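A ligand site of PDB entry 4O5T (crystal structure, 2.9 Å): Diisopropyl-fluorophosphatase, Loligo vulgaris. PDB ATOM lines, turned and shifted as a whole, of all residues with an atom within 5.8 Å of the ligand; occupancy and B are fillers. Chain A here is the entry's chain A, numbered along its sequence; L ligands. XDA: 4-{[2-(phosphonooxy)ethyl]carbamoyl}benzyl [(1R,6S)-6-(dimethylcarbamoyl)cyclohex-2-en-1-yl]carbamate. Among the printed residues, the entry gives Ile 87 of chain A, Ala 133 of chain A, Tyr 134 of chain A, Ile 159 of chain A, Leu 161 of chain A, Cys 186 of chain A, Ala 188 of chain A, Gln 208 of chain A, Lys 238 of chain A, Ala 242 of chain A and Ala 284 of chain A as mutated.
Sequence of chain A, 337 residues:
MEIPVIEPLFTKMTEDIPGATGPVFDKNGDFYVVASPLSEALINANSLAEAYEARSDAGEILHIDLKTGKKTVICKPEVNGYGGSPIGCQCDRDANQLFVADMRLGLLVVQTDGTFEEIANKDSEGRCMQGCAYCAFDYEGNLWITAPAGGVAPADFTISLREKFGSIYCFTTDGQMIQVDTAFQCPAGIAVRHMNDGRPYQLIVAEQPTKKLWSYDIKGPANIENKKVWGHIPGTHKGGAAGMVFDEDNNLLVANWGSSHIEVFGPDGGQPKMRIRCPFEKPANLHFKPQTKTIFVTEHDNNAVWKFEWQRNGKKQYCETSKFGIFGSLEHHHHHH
OG of Ser 39 touches C10 of the ligand, at 3.9 Å.
Leu 42 touches the ligand (O to C18, 3.6 Å).
Ala 45 touches the ligand (O to C27, 3.7 Å).
CG2 of Ile 87 touches C5 of the ligand (3.97 Å).
Met 103 touches the ligand.
Leu 161 touches the ligand (CD2 to O24, 3.5 Å).
Cys 186 touches the ligand.
Trp 257 touches the ligand (CD1 to C11, 3.2 Å).
Hydrophobic or aromatic side chains that line the ligand: Ile 87, Met 103, Leu 161 and Trp 257.
Within 4 Å of the ligand: Ser 39, Leu 42, Ala 45, Ile 87, Met 103, Tyr 134, Leu 161, Cys 186, Gln 208, Lys 238 and Trp 257.
O of Cys 186 sits at hydrogen-bond distance from N of Gln 208 (2.9 Å).
The indole nitrogen (NE1) of Trp 257 sits at hydrogen-bond distance from a ring nitrogen (ND1) of His 300 (3.3 Å).
OH of Tyr 134 lies within hydrogen-bond range of O8 of the ligand (3.0 Å).
An oxygen (O15) of the ligand sits close to the side-chain amide oxygen of Gln 208 (3.0 Å).
The side-chain amino group (NZ) of Lys 238 is in salt-bridge range of an oxygen (O31) of the ligand, at 3.8 Å.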
ATOM      1  N   SER A  39     -15.919 -16.758 -18.721  1.00  0.00           N
ATOM      2  CA  SER A  39     -15.552 -17.099 -20.091  1.00  0.00           C
ATOM      3  C   SER A  39     -16.220 -16.104 -20.994  1.00  0.00           C
ATOM      4  O   SER A  39     -15.572 -15.504 -21.821  1.00  0.00           O
ATOM      5  CB  SER A  39     -15.970 -18.545 -20.406  1.00  0.00           C
ATOM      6  OG  SER A  39     -15.127 -19.137 -21.368  1.00  0.00           O
ATOM      7  N   LEU A  42     -14.550 -12.698 -20.778  1.00  0.00           N
ATOM      8  CA  LEU A  42     -13.247 -12.612 -21.458  1.00  0.00           C
ATOM      9  C   LEU A  42     -13.402 -12.453 -22.977  1.00  0.00           C
ATOM     10  O   LEU A  42     -12.569 -11.817 -23.638  1.00  0.00           O
ATOM     11  CB  LEU A  42     -12.435 -13.890 -21.231  1.00  0.00           C
ATOM     12  CG  LEU A  42     -11.498 -13.936 -20.026  1.00  0.00           C
ATOM     13  CD1 LEU A  42     -11.229 -15.374 -19.588  1.00  0.00           C
ATOM     14  CD2 LEU A  42     -10.192 -13.215 -20.339  1.00  0.00           C
ATOM     15  N   ILE A  43     -14.483 -12.998 -23.503  1.00  0.00           N
ATOM     16  CA  ILE A  43     -14.813 -12.864 -24.909  1.00  0.00           C
ATOM     17  C   ILE A  43     -15.280 -11.455 -25.285  1.00  0.00           C
ATOM     18  O   ILE A  43     -14.958 -10.927 -26.341  1.00  0.00           O
ATOM     19  CB  ILE A  43     -15.866 -13.913 -25.339  1.00  0.00           C
ATOM     20  CG1 ILE A  43     -15.330 -15.335 -25.109  1.00  0.00           C
ATOM     21  CG2 ILE A  43     -16.248 -13.740 -26.805  1.00  0.00           C
ATOM     22  CD1 ILE A  43     -16.395 -16.400 -24.991  1.00  0.00           C
ATOM     23  N   ALA A  45     -14.600  -8.617 -23.604  1.00  0.00           N
ATOM     24  CA  ALA A  45     -13.692  -7.570 -23.134  1.00  0.00           C
ATOM     25  C   ALA A  45     -12.660  -7.181 -24.188  1.00  0.00           C
ATOM     26  O   ALA A  45     -12.426  -7.927 -25.127  1.00  0.00           O
ATOM     27  CB  ALA A  45     -12.985  -8.046 -21.870  1.00  0.00           C
ATOM     28  N   ASN A  46     -12.062  -6.007 -23.996  1.00  0.00           N
ATOM     29  CA  ASN A  46     -10.954  -5.549 -24.832  1.00  0.00           C
ATOM     30  C   ASN A  46      -9.587  -5.588 -24.128  1.00  0.00           C
ATOM     31  O   ASN A  46      -8.672  -4.873 -24.541  1.00  0.00           O
ATOM     32  CB  ASN A  46     -11.255  -4.131 -25.345  1.00  0.00           C
ATOM     33  N   SER A  47      -9.440  -6.386 -23.066  1.00  0.00           N
ATOM     34  CA  SER A  47      -8.123  -6.774 -22.525  1.00  0.00           C
ATOM     35  C   SER A  47      -8.093  -7.065 -21.014  1.00  0.00           C
ATOM     36  O   SER A  47      -8.306  -8.209 -20.590  1.00  0.00           O
ATOM     37  CB  SER A  47      -7.047  -5.737 -22.882  1.00  0.00           C
ATOM     38  N   ILE A  87     -14.576 -25.063 -16.077  1.00  0.00           N
ATOM     39  CA  ILE A  87     -14.450 -24.974 -17.509  1.00  0.00           C
ATOM     40  C   ILE A  87     -14.441 -26.311 -18.136  1.00  0.00           C
ATOM     41  O   ILE A  87     -14.823 -26.374 -19.313  1.00  0.00           O
ATOM     42  CB  ILE A  87     -13.217 -24.143 -17.953  1.00  0.00           C
ATOM     43  CG1 ILE A  87     -13.295 -22.689 -17.464  1.00  0.00           C
ATOM     44  CG2 ILE A  87     -13.075 -24.106 -19.472  1.00  0.00           C
ATOM     45  CD1 ILE A  87     -14.373 -21.838 -18.118  1.00  0.00           C
ATOM     46  N   MET A 103     -10.956 -22.458 -13.104  1.00  0.00           N
ATOM     47  CA  MET A 103      -9.894 -21.510 -13.346  1.00  0.00           C
ATOM     48  C   MET A 103      -9.586 -20.666 -12.122  1.00  0.00           C
ATOM     49  O   MET A 103      -8.543 -20.017 -12.061  1.00  0.00           O
ATOM     50  CB  MET A 103     -10.241 -20.553 -14.479  1.00  0.00           C
ATOM     51  CG  MET A 103     -10.476 -21.227 -15.807  1.00  0.00           C
ATOM     52  SD  MET A 103     -10.480 -19.989 -17.107  1.00  0.00           S
ATOM     53  CE  MET A 103      -8.714 -19.745 -17.305  1.00  0.00           C
ATOM     54  N   ALA A 133      -8.315 -25.603 -16.511  1.00  0.00           N
ATOM     55  CA  ALA A 133      -9.333 -25.398 -17.549  1.00  0.00           C
ATOM     56  C   ALA A 133      -9.839 -26.737 -18.072  1.00  0.00           C
ATOM     57  O   ALA A 133     -11.026 -27.017 -18.025  1.00  0.00           O
ATOM     58  CB  ALA A 133      -8.757 -24.574 -18.682  1.00  0.00           C
ATOM     59  N   TYR A 134      -8.951 -27.578 -18.576  1.00  0.00           N
ATOM     60  CA  TYR A 134      -9.394 -28.808 -19.282  1.00  0.00           C
ATOM     61  C   TYR A 134      -8.731 -29.993 -18.625  1.00  0.00           C
ATOM     62  O   TYR A 134      -7.745 -29.827 -17.976  1.00  0.00           O
ATOM     63  CB  TYR A 134      -9.081 -28.775 -20.771  1.00  0.00           C
ATOM     64  CG  TYR A 134      -9.840 -27.728 -21.575  1.00  0.00           C
ATOM     65  CD1 TYR A 134      -9.308 -26.454 -21.768  1.00  0.00           C
ATOM     66  CD2 TYR A 134     -11.068 -28.017 -22.161  1.00  0.00           C
ATOM     67  CE1 TYR A 134      -9.986 -25.503 -22.516  1.00  0.00           C
ATOM     68  CE2 TYR A 134     -11.747 -27.066 -22.909  1.00  0.00           C
ATOM     69  CZ  TYR A 134     -11.201 -25.811 -23.086  1.00  0.00           C
ATOM     70  OH  TYR A 134     -11.870 -24.856 -23.825  1.00  0.00           O
ATOM     71  N   PRO A 148      -4.218 -22.779 -17.663  1.00  0.00           N
ATOM     72  CA  PRO A 148      -3.866 -21.522 -18.325  1.00  0.00           C
ATOM     73  C   PRO A 148      -3.897 -20.275 -17.439  1.00  0.00           C
ATOM     74  O   PRO A 148      -3.455 -19.207 -17.890  1.00  0.00           O
ATOM     75  CB  PRO A 148      -4.892 -21.429 -19.452  1.00  0.00           C
ATOM     76  CG  PRO A 148      -6.085 -22.180 -18.957  1.00  0.00           C
ATOM     77  CD  PRO A 148      -5.641 -23.112 -17.860  1.00  0.00           C
ATOM     78  N   ILE A 159      -4.854 -14.889 -17.030  1.00  0.00           N
ATOM     79  CA  ILE A 159      -4.744 -16.011 -17.955  1.00  0.00           C
ATOM     80  C   ILE A 159      -3.633 -15.770 -19.001  1.00  0.00           C
ATOM     81  O   ILE A 159      -3.401 -14.624 -19.413  1.00  0.00           O
ATOM     82  CB  ILE A 159      -6.105 -16.288 -18.642  1.00  0.00           C
ATOM     83  CG1 ILE A 159      -6.106 -17.672 -19.282  1.00  0.00           C
ATOM     84  CG2 ILE A 159      -6.415 -15.225 -19.680  1.00  0.00           C
ATOM     85  CD1 ILE A 159      -7.424 -18.060 -19.902  1.00  0.00           C
ATOM     86  N   LEU A 161      -3.013 -15.807 -22.022  1.00  0.00           N
ATOM     87  CA  LEU A 161      -3.441 -15.656 -23.391  1.00  0.00           C
ATOM     88  C   LEU A 161      -2.448 -14.864 -24.195  1.00  0.00           C
ATOM     89  O   LEU A 161      -2.412 -15.006 -25.408  1.00  0.00           O
ATOM     90  CB  LEU A 161      -4.780 -14.977 -23.432  1.00  0.00           C
ATOM     91  CG  LEU A 161      -5.709 -15.751 -24.353  1.00  0.00           C
ATOM     92  CD1 LEU A 161      -7.109 -15.698 -23.751  1.00  0.00           C
ATOM     93  CD2 LEU A 161      -5.622 -15.203 -25.779  1.00  0.00           C
ATOM     94  N   CYS A 186      -1.555 -20.301 -22.918  1.00  0.00           N
ATOM     95  CA  CYS A 186      -2.978 -20.640 -22.861  1.00  0.00           C
ATOM     96  C   CYS A 186      -3.218 -22.050 -23.388  1.00  0.00           C
ATOM     97  O   CYS A 186      -3.812 -22.267 -24.476  1.00  0.00           O
ATOM     98  CB  CYS A 186      -3.841 -19.615 -23.595  1.00  0.00           C
ATOM     99  SG  CYS A 186      -5.597 -19.787 -23.158  1.00  0.00           S
ATOM    100  N   PRO A 187      -2.694 -23.020 -22.624  1.00  0.00           N
ATOM    101  CA  PRO A 187      -3.001 -24.389 -22.874  1.00  0.00           C
ATOM    102  C   PRO A 187      -4.508 -24.609 -22.683  1.00  0.00           C
ATOM    103  O   PRO A 187      -5.093 -24.069 -21.754  1.00  0.00           O
ATOM    104  CB  PRO A 187      -2.177 -25.147 -21.841  1.00  0.00           C
ATOM    105  CG  PRO A 187      -2.046 -24.203 -20.715  1.00  0.00           C
ATOM    106  CD  PRO A 187      -1.961 -22.855 -21.350  1.00  0.00           C
ATOM    107  N   ALA A 188      -5.140 -25.354 -23.587  1.00  0.00           N
ATOM    108  CA  ALA A 188      -6.603 -25.449 -23.618  1.00  0.00           C
ATOM    109  C   ALA A 188      -6.963 -26.920 -23.625  1.00  0.00           C
ATOM    110  O   ALA A 188      -6.616 -27.633 -22.673  1.00  0.00           O
ATOM    111  CB  ALA A 188      -7.130 -24.724 -24.856  1.00  0.00           C
ATOM    112  N   GLN A 208      -3.787 -22.601 -27.394  1.00  0.00           N
ATOM    113  CA  GLN A 208      -4.862 -22.033 -28.189  1.00  0.00           C
ATOM    114  C   GLN A 208      -4.505 -20.884 -29.205  1.00  0.00           C
ATOM    115  O   GLN A 208      -4.655 -21.052 -30.409  1.00  0.00           O
ATOM    116  CB  GLN A 208      -5.996 -21.594 -27.257  1.00  0.00           C
ATOM    117  CG  GLN A 208      -7.191 -20.973 -27.966  1.00  0.00           C
ATOM    118  CD  GLN A 208      -8.372 -20.778 -27.038  1.00  0.00           C
ATOM    119  OE1 GLN A 208      -9.040 -19.748 -27.083  1.00  0.00           O
ATOM    120  NE2 GLN A 208      -8.635 -21.762 -26.187  1.00  0.00           N
ATOM    121  N   LYS A 238      -8.914 -14.715 -34.220  1.00  0.00           N
ATOM    122  CA  LYS A 238      -8.908 -14.706 -32.752  1.00  0.00           C
ATOM    123  C   LYS A 238      -9.450 -16.065 -32.306  1.00  0.00           C
ATOM    124  O   LYS A 238     -10.557 -16.441 -32.660  1.00  0.00           O
ATOM    125  CB  LYS A 238      -9.796 -13.601 -32.195  1.00  0.00           C
ATOM    126  CG  LYS A 238      -9.818 -13.570 -30.667  1.00  0.00           C
ATOM    127  CD  LYS A 238     -11.146 -13.100 -30.088  1.00  0.00           C
ATOM    128  CE  LYS A 238     -11.150 -11.608 -29.761  1.00  0.00           C
ATOM    129  NZ  LYS A 238     -12.056 -11.307 -28.621  1.00  0.00           N
ATOM    130  N   GLY A 239      -8.660 -16.781 -31.518  1.00  0.00           N
ATOM    131  CA  GLY A 239      -9.066 -18.109 -31.032  1.00  0.00           C
ATOM    132  C   GLY A 239      -8.051 -19.168 -31.391  1.00  0.00           C
ATOM    133  O   GLY A 239      -6.836 -18.925 -31.355  1.00  0.00           O
ATOM    134  N   ALA A 242      -9.819 -25.214 -28.830  1.00  0.00           N
ATOM    135  CA  ALA A 242     -10.342 -25.274 -27.476  1.00  0.00           C
ATOM    136  C   ALA A 242     -10.496 -26.730 -27.038  1.00  0.00           C
ATOM    137  O   ALA A 242      -9.501 -27.409 -26.855  1.00  0.00           O
ATOM    138  CB  ALA A 242     -11.658 -24.532 -27.400  1.00  0.00           C
ATOM    139  N   TRP A 257     -12.071 -22.666 -32.115  1.00  0.00           N
ATOM    140  CA  TRP A 257     -12.904 -21.549 -31.712  1.00  0.00           C
ATOM    141  C   TRP A 257     -12.566 -20.340 -32.569  1.00  0.00           C
ATOM    142  O   TRP A 257     -11.392 -20.012 -32.696  1.00  0.00           O
ATOM    143  CB  TRP A 257     -12.618 -21.243 -30.244  1.00  0.00           C
ATOM    144  CG  TRP A 257     -13.566 -20.273 -29.600  1.00  0.00           C
ATOM    145  CD1 TRP A 257     -14.624 -20.586 -28.793  1.00  0.00           C
ATOM    146  CD2 TRP A 257     -13.532 -18.851 -29.697  1.00  0.00           C
ATOM    147  NE1 TRP A 257     -15.251 -19.440 -28.387  1.00  0.00           N
ATOM    148  CE2 TRP A 257     -14.602 -18.358 -28.914  1.00  0.00           C
ATOM    149  CE3 TRP A 257     -12.707 -17.936 -30.357  1.00  0.00           C
ATOM    150  CZ2 TRP A 257     -14.868 -16.997 -28.792  1.00  0.00           C
ATOM    151  CZ3 TRP A 257     -12.967 -16.592 -30.233  1.00  0.00           C
ATOM    152  CH2 TRP A 257     -14.045 -16.133 -29.448  1.00  0.00           C
ATOM    153  N   PRO A 283     -17.299 -22.816 -31.999  1.00  0.00           N
ATOM    154  CA  PRO A 283     -17.391 -24.043 -31.191  1.00  0.00           C
ATOM    155  C   PRO A 283     -16.357 -23.984 -30.074  1.00  0.00           C
ATOM    156  O   PRO A 283     -15.185 -23.640 -30.331  1.00  0.00           O
ATOM    157  CB  PRO A 283     -17.041 -25.150 -32.193  1.00  0.00           C
ATOM    158  CG  PRO A 283     -16.161 -24.472 -33.189  1.00  0.00           C
ATOM    159  CD  PRO A 283     -16.649 -23.052 -33.300  1.00  0.00           C
ATOM    160  N   ALA A 284     -16.749 -24.362 -28.857  1.00  0.00           N
ATOM    161  CA  ALA A 284     -15.845 -24.303 -27.675  1.00  0.00           C
ATOM    162  C   ALA A 284     -15.412 -25.658 -27.072  1.00  0.00           C
ATOM    163  O   ALA A 284     -14.264 -25.844 -26.649  1.00  0.00           O
ATOM    164  CB  ALA A 284     -16.491 -23.454 -26.602  1.00  0.00           C
ATOM    165  N   HIS A 300     -20.285 -20.429 -28.506  1.00  0.00           N
ATOM    166  CA  HIS A 300     -20.283 -19.137 -27.828  1.00  0.00           C
ATOM    167  C   HIS A 300     -20.858 -18.022 -28.688  1.00  0.00           C
ATOM    168  O   HIS A 300     -20.755 -16.864 -28.301  1.00  0.00           O
ATOM    169  CB  HIS A 300     -18.886 -18.793 -27.288  1.00  0.00           C
ATOM    170  CG  HIS A 300     -18.439 -19.691 -26.166  1.00  0.00           C
ATOM    171  ND1 HIS A 300     -17.147 -19.717 -25.695  1.00  0.00           N
ATOM    172  CD2 HIS A 300     -19.121 -20.601 -25.431  1.00  0.00           C
ATOM    173  CE1 HIS A 300     -17.044 -20.598 -24.720  1.00  0.00           C
ATOM    174  NE2 HIS A 300     -18.229 -21.148 -24.537  1.00  0.00           N
HETATM  175  O8  XDA L   1     -11.553 -21.929 -24.061  1.00  0.00           O
HETATM  176  C7  XDA L   1     -11.907 -20.772 -23.898  1.00  0.00           C
HETATM  177  N9  XDA L   1     -12.621 -20.135 -24.842  1.00  0.00           N
HETATM  178  C11 XDA L   1     -12.932 -20.739 -26.124  1.00  0.00           C
HETATM  179  C10 XDA L   1     -13.194 -18.800 -24.737  1.00  0.00           C
HETATM  180  C4  XDA L   1     -11.519 -20.043 -22.642  1.00  0.00           C
HETATM  181  C5  XDA L   1     -11.640 -20.960 -21.429  1.00  0.00           C
HETATM  182  C6  XDA L   1     -10.327 -21.188 -20.683  1.00  0.00           C
HETATM  183  C1  XDA L   1      -9.188 -21.364 -21.640  1.00  0.00           C
HETATM  184  C2  XDA L   1      -9.086 -20.544 -22.668  1.00  0.00           C
HETATM  185  C3  XDA L   1     -10.119 -19.462 -22.862  1.00  0.00           C
HETATM  186  N12 XDA L   1     -10.003 -18.894 -24.201  1.00  0.00           N
HETATM  187  C13 XDA L   1     -10.552 -17.730 -24.566  1.00  0.00           C
HETATM  188  O14 XDA L   1     -11.189 -17.023 -23.805  1.00  0.00           O
HETATM  189  O15 XDA L   1     -10.405 -17.351 -25.968  1.00  0.00           O
HETATM  190  C16 XDA L   1     -11.125 -16.251 -26.542  1.00  0.00           C
HETATM  191  C17 XDA L   1     -10.261 -15.027 -26.469  1.00  0.00           C
HETATM  192  C22 XDA L   1      -9.253 -14.856 -27.404  1.00  0.00           C
HETATM  193  C21 XDA L   1      -8.431 -13.738 -27.348  1.00  0.00           C
HETATM  194  C18 XDA L   1     -10.441 -14.082 -25.462  1.00  0.00           C
HETATM  195  C19 XDA L   1      -9.619 -12.956 -25.397  1.00  0.00           C
HETATM  196  C20 XDA L   1      -8.617 -12.783 -26.348  1.00  0.00           C
HETATM  197  C23 XDA L   1      -7.683 -11.606 -26.314  1.00  0.00           C
HETATM  198  O24 XDA L   1      -6.496 -11.875 -26.331  1.00  0.00           O
HETATM  199  N25 XDA L   1      -8.066 -10.326 -26.280  1.00  0.00           N
HETATM  200  C26 XDA L   1      -9.433  -9.852 -26.319  1.00  0.00           C
HETATM  201  C27 XDA L   1      -9.501  -8.630 -27.227  1.00  0.00           C
HETATM  202  O28 XDA L   1      -8.955  -9.007 -28.488  1.00  0.00           O
HETATM  203  P29 XDA L   1      -9.302  -8.180 -29.824  1.00  0.00           P
HETATM  204  O31 XDA L   1     -10.779  -7.872 -29.723  1.00  0.00           O
HETATM  205  O30 XDA L   1      -8.392  -6.974 -29.736  1.00  0.00           O
HETATM  206  O32 XDA L   1      -8.949  -9.119 -30.953  1.00  0.00           O
